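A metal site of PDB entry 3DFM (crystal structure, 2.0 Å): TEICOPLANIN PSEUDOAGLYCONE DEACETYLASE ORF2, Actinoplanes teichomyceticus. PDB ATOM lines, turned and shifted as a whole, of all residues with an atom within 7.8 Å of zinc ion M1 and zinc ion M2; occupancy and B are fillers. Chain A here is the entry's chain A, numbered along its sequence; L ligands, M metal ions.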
ATOM      1  N   SER A  14      23.918   5.387   1.744  1.00  0.00           N
ATOM      2  CA  SER A  14      23.706   4.594   0.536  1.00  0.00           C
ATOM      3  C   SER A  14      24.322   5.311  -0.674  1.00  0.00           C
ATOM      4  O   SER A  14      24.126   6.514  -0.856  1.00  0.00           O
ATOM      5  CB  SER A  14      22.199   4.418   0.323  1.00  0.00           C
ATOM      6  OG  SER A  14      21.910   3.521  -0.724  1.00  0.00           O
ATOM      7  N   PRO A  15      25.087   4.585  -1.510  1.00  0.00           N
ATOM      8  CA  PRO A  15      25.600   5.261  -2.709  1.00  0.00           C
ATOM      9  C   PRO A  15      24.451   5.678  -3.629  1.00  0.00           C
ATOM     10  O   PRO A  15      24.376   6.830  -4.045  1.00  0.00           O
ATOM     11  CB  PRO A  15      26.485   4.211  -3.374  1.00  0.00           C
ATOM     12  CG  PRO A  15      26.718   3.165  -2.328  1.00  0.00           C
ATOM     13  CD  PRO A  15      25.512   3.177  -1.447  1.00  0.00           C
ATOM     14  N   HIS A  16      23.535   4.745  -3.909  1.00  0.00           N
ATOM     15  CA  HIS A  16      22.471   4.999  -4.869  1.00  0.00           C
ATOM     16  C   HIS A  16      21.122   4.799  -4.215  1.00  0.00           C
ATOM     17  O   HIS A  16      21.024   4.170  -3.166  1.00  0.00           O
ATOM     18  CB  HIS A  16      22.557   4.028  -6.077  1.00  0.00           C
ATOM     19  CG  HIS A  16      23.851   4.095  -6.840  1.00  0.00           C
ATOM     20  ND1 HIS A  16      24.750   3.050  -6.864  1.00  0.00           N
ATOM     21  CD2 HIS A  16      24.378   5.072  -7.609  1.00  0.00           C
ATOM     22  CE1 HIS A  16      25.783   3.396  -7.622  1.00  0.00           C
ATOM     23  NE2 HIS A  16      25.576   4.609  -8.086  1.00  0.00           N
ATOM     24  N   LEU A  17      20.082   5.296  -4.866  1.00  0.00           N
ATOM     25  CA  LEU A  17      18.713   5.081  -4.451  1.00  0.00           C
ATOM     26  C   LEU A  17      18.326   3.612  -4.677  1.00  0.00           C
ATOM     27  O   LEU A  17      17.928   3.242  -5.774  1.00  0.00           O
ATOM     28  CB  LEU A  17      17.787   6.029  -5.235  1.00  0.00           C
ATOM     29  CG  LEU A  17      18.060   7.536  -5.026  1.00  0.00           C
ATOM     30  CD1 LEU A  17      17.521   8.405  -6.147  1.00  0.00           C
ATOM     31  CD2 LEU A  17      17.501   8.037  -3.658  1.00  0.00           C
ATOM     32  N   ASP A  18      18.508   2.799  -3.645  1.00  0.00           N
ATOM     33  CA  ASP A  18      18.153   1.361  -3.566  1.00  0.00           C
ATOM     34  C   ASP A  18      19.161   0.504  -2.803  1.00  0.00           C
ATOM     35  O   ASP A  18      18.800  -0.548  -2.294  1.00  0.00           O
ATOM     36  CB  ASP A  18      17.764   0.724  -4.934  1.00  0.00           C
ATOM     37  CG  ASP A  18      18.939   0.584  -5.897  1.00  0.00           C
ATOM     38  OD1 ASP A  18      20.075   1.012  -5.591  1.00  0.00           O
ATOM     39  OD2 ASP A  18      18.710   0.030  -7.007  1.00  0.00           O
ATOM     40  N   ASP A  19      20.417   0.945  -2.719  1.00  0.00           N
ATOM     41  CA  ASP A  19      21.475   0.112  -2.116  1.00  0.00           C
ATOM     42  C   ASP A  19      21.271  -0.242  -0.633  1.00  0.00           C
ATOM     43  O   ASP A  19      21.487  -1.372  -0.225  1.00  0.00           O
ATOM     44  CB  ASP A  19      22.844   0.772  -2.277  1.00  0.00           C
ATOM     45  CG  ASP A  19      23.310   0.827  -3.702  1.00  0.00           C
ATOM     46  OD1 ASP A  19      23.202  -0.191  -4.420  1.00  0.00           O
ATOM     47  OD2 ASP A  19      23.776   1.896  -4.113  1.00  0.00           O
ATOM     48  N   ALA A  20      20.884   0.753   0.175  1.00  0.00           N
ATOM     49  CA  ALA A  20      20.629   0.537   1.606  1.00  0.00           C
ATOM     50  C   ALA A  20      19.501  -0.464   1.800  1.00  0.00           C
ATOM     51  O   ALA A  20      19.586  -1.336   2.655  1.00  0.00           O
ATOM     52  CB  ALA A  20      20.276   1.864   2.299  1.00  0.00           C
ATOM     53  N   LEU A  22      18.258  -2.773  -0.428  1.00  0.00           N
ATOM     54  CA  LEU A  22      18.690  -4.091  -0.946  1.00  0.00           C
ATOM     55  C   LEU A  22      19.659  -4.830  -0.017  1.00  0.00           C
ATOM     56  O   LEU A  22      19.539  -6.049   0.185  1.00  0.00           O
ATOM     57  CB  LEU A  22      19.366  -3.904  -2.312  1.00  0.00           C
ATOM     58  CG  LEU A  22      18.448  -3.607  -3.505  1.00  0.00           C
ATOM     59  CD1 LEU A  22      19.256  -2.969  -4.622  1.00  0.00           C
ATOM     60  CD2 LEU A  22      17.774  -4.901  -3.993  1.00  0.00           C
ATOM     61  N   PHE A  44      24.478   9.759  -4.080  1.00  0.00           N
ATOM     62  CA  PHE A  44      24.274  10.066  -5.488  1.00  0.00           C
ATOM     63  C   PHE A  44      22.801  10.213  -5.881  1.00  0.00           C
ATOM     64  O   PHE A  44      22.275   9.477  -6.704  1.00  0.00           O
ATOM     65  CB  PHE A  44      25.075   9.094  -6.408  1.00  0.00           C
ATOM     66  CG  PHE A  44      26.541   9.221  -6.216  1.00  0.00           C
ATOM     67  CD1 PHE A  44      27.235  10.253  -6.805  1.00  0.00           C
ATOM     68  CD2 PHE A  44      27.205   8.367  -5.352  1.00  0.00           C
ATOM     69  CE1 PHE A  44      28.589  10.415  -6.585  1.00  0.00           C
ATOM     70  CE2 PHE A  44      28.584   8.516  -5.129  1.00  0.00           C
ATOM     71  CZ  PHE A  44      29.268   9.542  -5.737  1.00  0.00           C
ATOM     72  N   ARG A  75      13.149   8.397  -9.349  1.00  0.00           N
ATOM     73  CA  ARG A  75      13.877   7.487  -8.458  1.00  0.00           C
ATOM     74  C   ARG A  75      13.892   7.949  -6.994  1.00  0.00           C
ATOM     75  O   ARG A  75      13.880   7.130  -6.076  1.00  0.00           O
ATOM     76  CB  ARG A  75      15.276   7.240  -9.010  1.00  0.00           C
ATOM     77  CG  ARG A  75      15.185   6.463 -10.328  1.00  0.00           C
ATOM     78  CD  ARG A  75      16.400   5.680 -10.636  1.00  0.00           C
ATOM     79  NE  ARG A  75      16.790   4.799  -9.541  1.00  0.00           N
ATOM     80  CZ  ARG A  75      17.998   4.248  -9.446  1.00  0.00           C
ATOM     81  NH1 ARG A  75      18.899   4.484 -10.391  1.00  0.00           N
ATOM     82  NH2 ARG A  75      18.293   3.463  -8.431  1.00  0.00           N
ATOM     83  N   LEU A  96      25.828  14.142  -8.182  1.00  0.00           N
ATOM     84  CA  LEU A  96      25.283  13.637  -9.435  1.00  0.00           C
ATOM     85  C   LEU A  96      25.790  12.227  -9.694  1.00  0.00           C
ATOM     86  O   LEU A  96      27.000  11.972  -9.651  1.00  0.00           O
ATOM     87  CB  LEU A  96      25.628  14.558 -10.608  1.00  0.00           C
ATOM     88  CG  LEU A  96      25.052  15.972 -10.656  1.00  0.00           C
ATOM     89  CD1 LEU A  96      25.654  16.776 -11.812  1.00  0.00           C
ATOM     90  CD2 LEU A  96      23.540  15.940 -10.744  1.00  0.00           C
ATOM     91  N   ASP A  97      24.876  11.300  -9.967  1.00  0.00           N
ATOM     92  CA  ASP A  97      25.281   9.948 -10.281  1.00  0.00           C
ATOM     93  C   ASP A  97      26.215   9.918 -11.494  1.00  0.00           C
ATOM     94  O   ASP A  97      26.209  10.839 -12.299  1.00  0.00           O
ATOM     95  CB  ASP A  97      24.058   9.062 -10.533  1.00  0.00           C
ATOM     96  CG  ASP A  97      24.396   7.598 -10.452  1.00  0.00           C
ATOM     97  OD1 ASP A  97      25.470   7.269  -9.902  1.00  0.00           O
ATOM     98  OD2 ASP A  97      23.608   6.784 -10.943  1.00  0.00           O
ATOM     99  N   SER A  98      27.012   8.850 -11.610  1.00  0.00           N
ATOM    100  CA  SER A  98      28.024   8.703 -12.672  1.00  0.00           C
ATOM    101  C   SER A  98      27.555   9.099 -14.094  1.00  0.00           C
ATOM    102  O   SER A  98      28.321   9.729 -14.836  1.00  0.00           O
ATOM    103  CB  SER A  98      28.578   7.271 -12.670  1.00  0.00           C
ATOM    104  OG  SER A  98      27.594   6.390 -13.158  1.00  0.00           O
ATOM    105  N   ILE A  99      26.335   8.743 -14.462  1.00  0.00           N
ATOM    106  CA  ILE A  99      25.826   8.997 -15.834  1.00  0.00           C
ATOM    107  C   ILE A  99      25.481  10.464 -16.103  1.00  0.00           C
ATOM    108  O   ILE A  99      25.154  10.839 -17.234  1.00  0.00           O
ATOM    109  CB  ILE A  99      24.552   8.149 -16.200  1.00  0.00           C
ATOM    110  CG1 ILE A  99      23.536   8.137 -15.044  1.00  0.00           C
ATOM    111  CG2 ILE A  99      24.921   6.717 -16.597  1.00  0.00           C
ATOM    112  CD1 ILE A  99      22.129   7.736 -15.477  1.00  0.00           C
ATOM    113  N   ARG A 101      27.597  13.054 -14.562  1.00  0.00           N
ATOM    114  CA  ARG A 101      28.800  13.845 -14.299  1.00  0.00           C
ATOM    115  C   ARG A 101      29.606  14.094 -15.577  1.00  0.00           C
ATOM    116  O   ARG A 101      29.624  13.264 -16.500  1.00  0.00           O
ATOM    117  CB  ARG A 101      29.693  13.162 -13.246  1.00  0.00           C
ATOM    118  CG  ARG A 101      29.004  12.963 -11.906  1.00  0.00           C
ATOM    119  CD  ARG A 101      29.988  12.786 -10.739  1.00  0.00           C
ATOM    120  NE  ARG A 101      30.767  11.544 -10.770  1.00  0.00           N
ATOM    121  CZ  ARG A 101      30.361  10.349 -10.352  1.00  0.00           C
ATOM    122  NH1 ARG A 101      29.137  10.172  -9.889  1.00  0.00           N
ATOM    123  NH2 ARG A 101      31.177   9.311 -10.404  1.00  0.00           N
ATOM    124  N   CYS A 155      28.263   1.050   2.579  1.00  0.00           N
ATOM    125  CA  CYS A 155      28.535  -0.122   1.715  1.00  0.00           C
ATOM    126  C   CYS A 155      30.004  -0.556   1.745  1.00  0.00           C
ATOM    127  O   CYS A 155      30.890   0.288   1.819  1.00  0.00           O
ATOM    128  CB  CYS A 155      28.155   0.210   0.257  1.00  0.00           C
ATOM    129  SG  CYS A 155      29.029   1.609  -0.441  1.00  0.00           S
ATOM    130  N   HIS A 161      31.986  -1.068  -7.651  1.00  0.00           N
ATOM    131  CA  HIS A 161      31.355   0.060  -8.314  1.00  0.00           C
ATOM    132  C   HIS A 161      32.031   1.369  -7.842  1.00  0.00           C
ATOM    133  O   HIS A 161      32.207   1.550  -6.642  1.00  0.00           O
ATOM    134  CB  HIS A 161      29.864   0.098  -8.001  1.00  0.00           C
ATOM    135  CG  HIS A 161      29.089   0.926  -8.953  1.00  0.00           C
ATOM    136  ND1 HIS A 161      29.269   2.288  -9.057  1.00  0.00           N
ATOM    137  CD2 HIS A 161      28.144   0.598  -9.855  1.00  0.00           C
ATOM    138  CE1 HIS A 161      28.467   2.765  -9.995  1.00  0.00           C
ATOM    139  NE2 HIS A 161      27.763   1.762 -10.487  1.00  0.00           N
ATOM    140  N   PRO A 162      32.466   2.238  -8.786  1.00  0.00           N
ATOM    141  CA  PRO A 162      33.188   3.457  -8.393  1.00  0.00           C
ATOM    142  C   PRO A 162      32.403   4.371  -7.453  1.00  0.00           C
ATOM    143  O   PRO A 162      32.988   4.974  -6.542  1.00  0.00           O
ATOM    144  CB  PRO A 162      33.465   4.149  -9.738  1.00  0.00           C
ATOM    145  CG  PRO A 162      33.437   3.040 -10.736  1.00  0.00           C
ATOM    146  CD  PRO A 162      32.353   2.120 -10.247  1.00  0.00           C
ATOM    147  N   ASP A 163      31.096   4.481  -7.664  1.00  0.00           N
ATOM    148  CA  ASP A 163      30.259   5.305  -6.775  1.00  0.00           C
ATOM    149  C   ASP A 163      30.097   4.685  -5.389  1.00  0.00           C
ATOM    150  O   ASP A 163      29.915   5.396  -4.412  1.00  0.00           O
ATOM    151  CB  ASP A 163      28.906   5.594  -7.413  1.00  0.00           C
ATOM    152  CG  ASP A 163      29.024   6.470  -8.663  1.00  0.00           C
ATOM    153  OD1 ASP A 163      30.038   7.176  -8.802  1.00  0.00           O
ATOM    154  OD2 ASP A 163      28.107   6.414  -9.505  1.00  0.00           O
ATOM    155  N   HIS A 164      30.169   3.352  -5.319  1.00  0.00           N
ATOM    156  CA  HIS A 164      30.168   2.642  -4.032  1.00  0.00           C
ATOM    157  C   HIS A 164      31.480   2.852  -3.273  1.00  0.00           C
ATOM    158  O   HIS A 164      31.499   3.044  -2.046  1.00  0.00           O
ATOM    159  CB  HIS A 164      29.889   1.150  -4.252  1.00  0.00           C
ATOM    160  CG  HIS A 164      28.459   0.840  -4.603  1.00  0.00           C
ATOM    161  ND1 HIS A 164      27.818  -0.315  -4.195  1.00  0.00           N
ATOM    162  CD2 HIS A 164      27.549   1.527  -5.318  1.00  0.00           C
ATOM    163  CE1 HIS A 164      26.584  -0.316  -4.635  1.00  0.00           C
ATOM    164  NE2 HIS A 164      26.382   0.799  -5.324  1.00  0.00           N
ATOM    165  N   THR A 167      31.595   6.495  -1.953  1.00  0.00           N
ATOM    166  CA  THR A 167      30.691   6.660  -0.811  1.00  0.00           C
ATOM    167  C   THR A 167      31.335   6.082   0.435  1.00  0.00           C
ATOM    168  O   THR A 167      31.394   6.742   1.474  1.00  0.00           O
ATOM    169  CB  THR A 167      29.339   5.953  -1.063  1.00  0.00           C
ATOM    170  OG1 THR A 167      28.674   6.592  -2.142  1.00  0.00           O
ATOM    171  CG2 THR A 167      28.445   6.032   0.172  1.00  0.00           C
ATOM    172  N   ASP A 187      27.325  -5.624  -0.024  1.00  0.00           N
ATOM    173  CA  ASP A 187      26.563  -5.070  -1.154  1.00  0.00           C
ATOM    174  C   ASP A 187      25.722  -6.138  -1.858  1.00  0.00           C
ATOM    175  O   ASP A 187      26.268  -7.143  -2.318  1.00  0.00           O
ATOM    176  CB  ASP A 187      27.477  -4.420  -2.196  1.00  0.00           C
ATOM    177  CG  ASP A 187      28.444  -3.402  -1.585  1.00  0.00           C
ATOM    178  OD1 ASP A 187      28.377  -2.211  -1.956  1.00  0.00           O
ATOM    179  OD2 ASP A 187      29.254  -3.800  -0.726  1.00  0.00           O
ATOM    180  N   LEU A 188      24.415  -5.919  -1.941  1.00  0.00           N
ATOM    181  CA  LEU A 188      23.526  -6.838  -2.667  1.00  0.00           C
ATOM    182  C   LEU A 188      22.793  -6.126  -3.800  1.00  0.00           C
ATOM    183  O   LEU A 188      22.456  -4.945  -3.670  1.00  0.00           O
ATOM    184  CB  LEU A 188      22.528  -7.497  -1.724  1.00  0.00           C
ATOM    185  CG  LEU A 188      23.062  -8.375  -0.593  1.00  0.00           C
ATOM    186  CD1 LEU A 188      21.890  -8.810   0.296  1.00  0.00           C
ATOM    187  CD2 LEU A 188      23.829  -9.577  -1.119  1.00  0.00           C
ATOM    188  N   TYR A 190      25.131  -7.515  -5.604  1.00  0.00           N
ATOM    189  CA  TYR A 190      26.530  -7.667  -6.029  1.00  0.00           C
ATOM    190  C   TYR A 190      27.213  -8.910  -5.481  1.00  0.00           C
ATOM    191  O   TYR A 190      27.861  -9.648  -6.241  1.00  0.00           O
ATOM    192  CB  TYR A 190      27.363  -6.436  -5.637  1.00  0.00           C
ATOM    193  CG  TYR A 190      27.016  -5.166  -6.382  1.00  0.00           C
ATOM    194  CD1 TYR A 190      27.721  -4.786  -7.526  1.00  0.00           C
ATOM    195  CD2 TYR A 190      25.979  -4.331  -5.941  1.00  0.00           C
ATOM    196  CE1 TYR A 190      27.414  -3.627  -8.213  1.00  0.00           C
ATOM    197  CE2 TYR A 190      25.657  -3.157  -6.634  1.00  0.00           C
ATOM    198  CZ  TYR A 190      26.385  -2.820  -7.761  1.00  0.00           C
ATOM    199  OH  TYR A 190      26.121  -1.673  -8.455  1.00  0.00           O
HETATM  200  S1  LIG L   1      25.164   3.792 -11.950  1.00  0.00           S
HETATM  201  O1  LIG L   1      24.583   4.442 -13.105  1.00  0.00           O
HETATM  202  O2  LIG L   1      26.195   4.645 -11.441  1.00  0.00           O
HETATM  203  O3  LIG L   1      24.038   3.517 -11.075  1.00  0.00           O
HETATM  204  O4  LIG L   1      25.798   2.557 -12.345  1.00  0.00           O
HETATM  205  S1  LG2 L   2      22.647  -0.338  -7.851  1.00  0.00           S
HETATM  206  O1  LG2 L   2      22.079  -1.484  -7.192  1.00  0.00           O
HETATM  207  O2  LG2 L   2      21.977   0.900  -7.502  1.00  0.00           O
HETATM  208  O3  LG2 L   2      24.070  -0.384  -7.577  1.00  0.00           O
HETATM  209  O4  LG2 L   2      22.567  -0.377  -9.300  1.00  0.00           O
HETATM  210 ZN    ZN M   1      26.397   5.663  -9.604  1.00  0.00          ZN
HETATM  211 ZN    ZN M   2      24.583   1.305  -6.065  1.00  0.00          ZN
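The backbone carbonyl oxygen of His 164 sits at hydrogen-bond distance from the side-chain sulfur of Cys 155. The backbone carbonyl oxygen (O) of Asp 163 sits at hydrogen-bond distance from the side-chain hydroxyl (OG1) of Thr 167 (2.9 Å). N of Asp 163 sits at hydrogen-bond distance from ND1 of His 161, at 3.2 Å. N of Ser 98 lies close to OD2 of Asp 163, at 3.4 Å. NH2 of Arg 101 is in salt-bridge range of OD1 of Asp 163 (2.9 Å). OD1 of Asp 187 lies within hydrogen-bond range of ND1 of His 164 (3.0 Å). OG of Ser 14 sits at hydrogen-bond distance from O of His 16, at 2.7 Å.
Ser 98 touches zinc ion M1 (N to ZN, 3.8 Å). CE1 of His 161 touches zinc ion M1 (3.6 Å). Five residues have an atom within 4 Å of zinc ion M1: His 16, Asp 97, Ser 98, His 161 and Asp 163.
Three residues have an atom within 4 Å of zinc ion M2: His 16, Asp 19 and His 164.
Zinc ion M1 is bound by the side-chain carboxylate (OD2) of Asp 163, 1.9 Å away. OD1 of Asp 97 binds zinc ion M1. Zinc ion M1 is bound by a ring nitrogen (NE2) of His 16 (2.0 Å). O2 of LIG L1 is bound to zinc ion M1 (2.1 Å). Zinc ion M1 has four donor atoms within binding distance.
Zinc ion M2 is bound by a ring nitrogen (ND1) of His 16, a ring nitrogen (NE2) of His 164, the side-chain carboxylate of Asp 19 and an oxygen (O3) of LG2 L2. Zinc ion M2 has four donor atoms within binding distance. Slightly farther from zinc ion M2 lies OD1 of Asp 19 (2.6 Å).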
